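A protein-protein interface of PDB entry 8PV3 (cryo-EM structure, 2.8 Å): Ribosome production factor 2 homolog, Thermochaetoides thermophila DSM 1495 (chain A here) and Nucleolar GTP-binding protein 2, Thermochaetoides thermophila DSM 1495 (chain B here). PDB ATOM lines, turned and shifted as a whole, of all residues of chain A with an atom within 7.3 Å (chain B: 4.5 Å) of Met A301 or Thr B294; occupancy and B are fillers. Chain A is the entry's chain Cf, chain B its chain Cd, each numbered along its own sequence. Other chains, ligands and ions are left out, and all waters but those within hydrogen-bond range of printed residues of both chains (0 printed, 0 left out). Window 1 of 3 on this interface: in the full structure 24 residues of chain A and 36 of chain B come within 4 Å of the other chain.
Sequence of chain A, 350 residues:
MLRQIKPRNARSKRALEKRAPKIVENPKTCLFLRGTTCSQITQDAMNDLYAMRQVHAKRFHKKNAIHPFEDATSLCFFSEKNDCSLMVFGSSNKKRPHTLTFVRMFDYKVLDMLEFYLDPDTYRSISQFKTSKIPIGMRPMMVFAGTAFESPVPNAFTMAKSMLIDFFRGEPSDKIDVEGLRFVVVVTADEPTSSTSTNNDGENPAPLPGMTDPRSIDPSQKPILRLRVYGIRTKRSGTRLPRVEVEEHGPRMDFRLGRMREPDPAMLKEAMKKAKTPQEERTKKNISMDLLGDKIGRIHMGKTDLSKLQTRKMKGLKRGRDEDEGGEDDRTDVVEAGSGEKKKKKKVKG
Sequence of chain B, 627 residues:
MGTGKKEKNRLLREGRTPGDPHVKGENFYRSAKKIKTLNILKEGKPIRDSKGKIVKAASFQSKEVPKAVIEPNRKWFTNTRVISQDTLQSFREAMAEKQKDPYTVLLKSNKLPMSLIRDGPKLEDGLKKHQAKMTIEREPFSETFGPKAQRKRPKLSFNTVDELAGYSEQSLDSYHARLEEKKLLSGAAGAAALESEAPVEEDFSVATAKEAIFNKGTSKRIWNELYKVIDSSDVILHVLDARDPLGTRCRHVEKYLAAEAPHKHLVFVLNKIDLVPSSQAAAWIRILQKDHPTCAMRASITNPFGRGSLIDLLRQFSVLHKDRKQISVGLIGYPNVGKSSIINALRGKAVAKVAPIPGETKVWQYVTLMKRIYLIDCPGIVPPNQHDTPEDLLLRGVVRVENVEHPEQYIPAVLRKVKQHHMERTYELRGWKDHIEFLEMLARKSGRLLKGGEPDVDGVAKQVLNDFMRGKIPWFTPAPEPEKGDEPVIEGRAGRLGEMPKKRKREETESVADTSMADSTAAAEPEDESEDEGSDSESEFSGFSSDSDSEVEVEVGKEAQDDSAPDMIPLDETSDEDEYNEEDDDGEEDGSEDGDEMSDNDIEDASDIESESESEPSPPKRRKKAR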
ATOM      1  N   ILE A 299     -32.535   8.607   1.110  1.00  0.00           N
ATOM      2  CA  ILE A 299     -31.691   7.654   1.818  1.00  0.00           C
ATOM      3  C   ILE A 299     -31.795   7.921   3.312  1.00  0.00           C
ATOM      4  O   ILE A 299     -31.737   9.067   3.771  1.00  0.00           O
ATOM      5  CB  ILE A 299     -30.224   7.701   1.342  1.00  0.00           C
ATOM      6  CG1 ILE A 299     -29.720   9.142   1.265  1.00  0.00           C
ATOM      7  CG2 ILE A 299     -30.080   7.006  -0.001  1.00  0.00           C
ATOM      8  CD1 ILE A 299     -28.272   9.257   0.864  1.00  0.00           C
ATOM      9  N   HIS A 300     -31.965   6.843   4.074  1.00  0.00           N
ATOM     10  CA  HIS A 300     -32.174   6.911   5.516  1.00  0.00           C
ATOM     11  C   HIS A 300     -30.912   6.416   6.208  1.00  0.00           C
ATOM     12  O   HIS A 300     -30.633   5.214   6.214  1.00  0.00           O
ATOM     13  CB  HIS A 300     -33.390   6.084   5.921  1.00  0.00           C
ATOM     14  CG  HIS A 300     -34.611   6.378   5.109  1.00  0.00           C
ATOM     15  ND1 HIS A 300     -35.429   7.459   5.357  1.00  0.00           N
ATOM     16  CD2 HIS A 300     -35.148   5.737   4.045  1.00  0.00           C
ATOM     17  CE1 HIS A 300     -36.421   7.468   4.485  1.00  0.00           C
ATOM     18  NE2 HIS A 300     -36.273   6.433   3.677  1.00  0.00           N
ATOM     19  N   MET A 301     -30.149   7.350   6.777  1.00  0.00           N
ATOM     20  CA  MET A 301     -28.886   6.995   7.419  1.00  0.00           C
ATOM     21  C   MET A 301     -29.113   6.297   8.754  1.00  0.00           C
ATOM     22  O   MET A 301     -28.482   5.275   9.047  1.00  0.00           O
ATOM     23  CB  MET A 301     -28.036   8.249   7.610  1.00  0.00           C
ATOM     24  CG  MET A 301     -27.580   8.883   6.315  1.00  0.00           C
ATOM     25  SD  MET A 301     -26.557   7.763   5.355  1.00  0.00           S
ATOM     26  CE  MET A 301     -25.107   7.720   6.397  1.00  0.00           C
ATOM     27  N   GLY A 302     -30.005   6.833   9.574  1.00  0.00           N
ATOM     28  CA  GLY A 302     -30.190   6.343  10.921  1.00  0.00           C
ATOM     29  C   GLY A 302     -29.231   6.996  11.905  1.00  0.00           C
ATOM     30  O   GLY A 302     -28.320   7.742  11.537  1.00  0.00           O
ATOM     31  N   LYS A 303     -29.446   6.706  13.183  1.00  0.00           N
ATOM     32  CA  LYS A 303     -28.616   7.280  14.232  1.00  0.00           C
ATOM     33  C   LYS A 303     -27.256   6.595  14.282  1.00  0.00           C
ATOM     34  O   LYS A 303     -27.142   5.386  14.066  1.00  0.00           O
ATOM     35  CB  LYS A 303     -29.313   7.161  15.587  1.00  0.00           C
ATOM     36  N   THR A 304     -26.220   7.382  14.567  1.00  0.00           N
ATOM     37  CA  THR A 304     -24.872   6.850  14.719  1.00  0.00           C
ATOM     38  C   THR A 304     -24.608   6.566  16.192  1.00  0.00           C
ATOM     39  O   THR A 304     -24.713   7.466  17.033  1.00  0.00           O
ATOM     40  CB  THR A 304     -23.841   7.831  14.167  1.00  0.00           C
ATOM     41  N   TYR B 103     -29.664  14.230   2.337  1.00  0.00           N
ATOM     42  CA  TYR B 103     -30.240  12.896   2.274  1.00  0.00           C
ATOM     43  C   TYR B 103     -31.127  12.692   1.054  1.00  0.00           C
ATOM     44  O   TYR B 103     -31.823  11.675   0.971  1.00  0.00           O
ATOM     45  CB  TYR B 103     -31.022  12.608   3.555  1.00  0.00           C
ATOM     46  CG  TYR B 103     -30.191  12.809   4.799  1.00  0.00           C
ATOM     47  CD1 TYR B 103     -28.950  12.199   4.930  1.00  0.00           C
ATOM     48  CD2 TYR B 103     -30.636  13.620   5.833  1.00  0.00           C
ATOM     49  CE1 TYR B 103     -28.179  12.387   6.058  1.00  0.00           C
ATOM     50  CE2 TYR B 103     -29.873  13.811   6.968  1.00  0.00           C
ATOM     51  CZ  TYR B 103     -28.646  13.191   7.074  1.00  0.00           C
ATOM     52  OH  TYR B 103     -27.880  13.378   8.201  1.00  0.00           O
ATOM     53  N   PHE B 268     -19.361  10.213   2.187  1.00  0.00           N
ATOM     54  CA  PHE B 268     -18.163  10.252   3.015  1.00  0.00           C
ATOM     55  C   PHE B 268     -18.063   8.993   3.863  1.00  0.00           C
ATOM     56  O   PHE B 268     -19.058   8.528   4.425  1.00  0.00           O
ATOM     57  CB  PHE B 268     -18.175  11.470   3.937  1.00  0.00           C
ATOM     58  CG  PHE B 268     -17.791  12.749   3.265  1.00  0.00           C
ATOM     59  CD1 PHE B 268     -16.656  12.825   2.482  1.00  0.00           C
ATOM     60  CD2 PHE B 268     -18.560  13.885   3.438  1.00  0.00           C
ATOM     61  CE1 PHE B 268     -16.304  14.007   1.871  1.00  0.00           C
ATOM     62  CE2 PHE B 268     -18.212  15.068   2.830  1.00  0.00           C
ATOM     63  CZ  PHE B 268     -17.083  15.130   2.047  1.00  0.00           C
ATOM     64  N   ILE B 285     -18.227  13.694  12.208  1.00  0.00           N
ATOM     65  CA  ILE B 285     -19.400  13.193  11.493  1.00  0.00           C
ATOM     66  C   ILE B 285     -20.461  14.280  11.387  1.00  0.00           C
ATOM     67  O   ILE B 285     -21.071  14.474  10.328  1.00  0.00           O
ATOM     68  CB  ILE B 285     -19.953  11.940  12.195  1.00  0.00           C
ATOM     69  CG1 ILE B 285     -19.047  10.738  11.966  1.00  0.00           C
ATOM     70  CG2 ILE B 285     -21.361  11.607  11.718  1.00  0.00           C
ATOM     71  CD1 ILE B 285     -19.420   9.581  12.840  1.00  0.00           C
ATOM     72  N   LEU B 288     -19.353  16.778   8.738  1.00  0.00           N
ATOM     73  CA  LEU B 288     -19.383  16.311   7.352  1.00  0.00           C
ATOM     74  C   LEU B 288     -20.801  16.023   6.862  1.00  0.00           C
ATOM     75  O   LEU B 288     -21.068  16.118   5.655  1.00  0.00           O
ATOM     76  CB  LEU B 288     -18.513  15.067   7.198  1.00  0.00           C
ATOM     77  CG  LEU B 288     -17.017  15.252   7.442  1.00  0.00           C
ATOM     78  CD1 LEU B 288     -16.349  13.903   7.624  1.00  0.00           C
ATOM     79  CD2 LEU B 288     -16.370  16.027   6.311  1.00  0.00           C
ATOM     80  N   GLN B 289     -21.718  15.668   7.768  1.00  0.00           N
ATOM     81  CA  GLN B 289     -23.088  15.365   7.371  1.00  0.00           C
ATOM     82  C   GLN B 289     -23.859  16.594   6.913  1.00  0.00           C
ATOM     83  O   GLN B 289     -24.922  16.441   6.304  1.00  0.00           O
ATOM     84  CB  GLN B 289     -23.833  14.686   8.519  1.00  0.00           C
ATOM     85  CG  GLN B 289     -23.558  13.198   8.628  1.00  0.00           C
ATOM     86  CD  GLN B 289     -24.475  12.502   9.611  1.00  0.00           C
ATOM     87  OE1 GLN B 289     -25.176  11.554   9.258  1.00  0.00           O
ATOM     88  NE2 GLN B 289     -24.475  12.969  10.853  1.00  0.00           N
ATOM     89  N   HIS B 292     -22.410  15.961   3.011  1.00  0.00           N
ATOM     90  CA  HIS B 292     -22.703  14.689   2.369  1.00  0.00           C
ATOM     91  C   HIS B 292     -22.971  13.630   3.427  1.00  0.00           C
ATOM     92  O   HIS B 292     -22.509  13.767   4.565  1.00  0.00           O
ATOM     93  CB  HIS B 292     -21.542  14.248   1.461  1.00  0.00           C
ATOM     94  CG  HIS B 292     -21.393  15.080   0.228  1.00  0.00           C
ATOM     95  ND1 HIS B 292     -20.528  16.151   0.152  1.00  0.00           N
ATOM     96  CD2 HIS B 292     -22.008  15.008  -0.975  1.00  0.00           C
ATOM     97  CE1 HIS B 292     -20.613  16.697  -1.047  1.00  0.00           C
ATOM     98  NE2 HIS B 292     -21.505  16.024  -1.750  1.00  0.00           N
ATOM     99  N   PRO B 293     -23.732  12.585   3.093  1.00  0.00           N
ATOM    100  CA  PRO B 293     -23.964  11.500   4.058  1.00  0.00           C
ATOM    101  C   PRO B 293     -22.668  10.808   4.451  1.00  0.00           C
ATOM    102  O   PRO B 293     -21.873  10.409   3.600  1.00  0.00           O
ATOM    103  CB  PRO B 293     -24.901  10.552   3.304  1.00  0.00           C
ATOM    104  CG  PRO B 293     -25.562  11.395   2.291  1.00  0.00           C
ATOM    105  CD  PRO B 293     -24.571  12.436   1.892  1.00  0.00           C
ATOM    106  N   THR B 294     -22.460  10.664   5.758  1.00  0.00           N
ATOM    107  CA  THR B 294     -21.188  10.223   6.308  1.00  0.00           C
ATOM    108  C   THR B 294     -21.375   8.951   7.120  1.00  0.00           C
ATOM    109  O   THR B 294     -22.297   8.852   7.935  1.00  0.00           O
ATOM    110  CB  THR B 294     -20.566  11.312   7.190  1.00  0.00           C
ATOM    111  OG1 THR B 294     -20.604  12.564   6.496  1.00  0.00           O
ATOM    112  CG2 THR B 294     -19.124  10.976   7.527  1.00  0.00           C
ATOM    113  N   CYS B 295     -20.493   7.980   6.892  1.00  0.00           N
ATOM    114  CA  CYS B 295     -20.452   6.746   7.661  1.00  0.00           C
ATOM    115  C   CYS B 295     -19.093   6.608   8.329  1.00  0.00           C
ATOM    116  O   CYS B 295     -18.059   6.724   7.670  1.00  0.00           O
ATOM    117  CB  CYS B 295     -20.705   5.521   6.775  1.00  0.00           C
ATOM    118  SG  CYS B 295     -22.275   5.513   5.895  1.00  0.00           S
ATOM    119  N   ALA B 296     -19.093   6.356   9.632  1.00  0.00           N
ATOM    120  CA  ALA B 296     -17.871   6.039  10.356  1.00  0.00           C
ATOM    121  C   ALA B 296     -17.599   4.549  10.244  1.00  0.00           C
ATOM    122  O   ALA B 296     -18.531   3.740  10.253  1.00  0.00           O
ATOM    123  CB  ALA B 296     -17.974   6.433  11.826  1.00  0.00           C
ATOM    124  N   LEU B 313     -26.725   1.172   3.590  1.00  0.00           N
ATOM    125  CA  LEU B 313     -26.761   2.331   2.699  1.00  0.00           C
ATOM    126  C   LEU B 313     -26.578   1.914   1.242  1.00  0.00           C
ATOM    127  O   LEU B 313     -27.265   2.424   0.343  1.00  0.00           O
ATOM    128  CB  LEU B 313     -25.694   3.342   3.117  1.00  0.00           C
ATOM    129  CG  LEU B 313     -25.696   4.674   2.368  1.00  0.00           C
ATOM    130  CD1 LEU B 313     -27.046   5.352   2.494  1.00  0.00           C
ATOM    131  CD2 LEU B 313     -24.593   5.579   2.886  1.00  0.00           C
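The side-chain amide oxygen (OE1) of Gln B289 lies within hydrogen-bond range of the side-chain hydroxyl (OH) of Tyr B103 (3.4 Å). The backbone carbonyl oxygen of Phe B268 is in hydrogen-bond range of the backbone NH of Cys B295, 2.9 Å away. N of Phe B268 is in hydrogen-bond range of O of Pro B293, at 2.9 Å. The backbone carbonyl oxygen of His B292 is in hydrogen-bond range of the side-chain hydroxyl of Thr B294 (3.0 Å).
Pro B293 touches Ile A299 (CG to CD1, 3.7 Å). Met A301 touches Tyr B103. Met A301 touches Pro B293 (SD to CB, 3.8 Å). Met A301 touches Thr B294 (CE to O, 3.4 Å). Cys B295 touches Met A301 (SG to CE, 3.6 Å). Met A301 touches Leu B313 (SD to CD1, 3.8 Å).
Of chain B, only Tyr B103, Pro B293, Thr B294, Cys B295 and Leu B313 come within 4 Å of Met A301. Printed residues of chain B within 4 Å of Ile A299: Tyr B103 (3.2 Å) and Pro B293 (3.7 Å). Printed residues of chain A within 4 Å of Tyr B103: Ile A299 (3.2 Å) and Met A301 (3.6 Å). Printed residues of chain A within 4 Å of Leu B313: Met A301. Ile B285 touches none of the printed residues of chain A. Thr A304 touches none of the printed residues of chain B. The nearest printed residue of chain A that does not touch Tyr B103 is His A300 (5.7 Å).
The backbone carbonyl oxygen (O) of Tyr B103 lies within hydrogen-bond range of the backbone NH (N) of Ile A299, 3.2 Å away.
Printed residues of chain A that touch a printed residue of chain B: Ile A299 and Met A301. Hydrophobic or aromatic side chains of chain A that line the printed part of chain B: Ile A299 and Met A301. Of the 11 printed residues of chain B, 5 touch a printed residue of chain A. Hydrophobic or aromatic side chains of chain B that line the printed part of chain A: Tyr B103, Pro B293 and Leu B313. Among the printed residues, 7 pairs touch across the chains.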
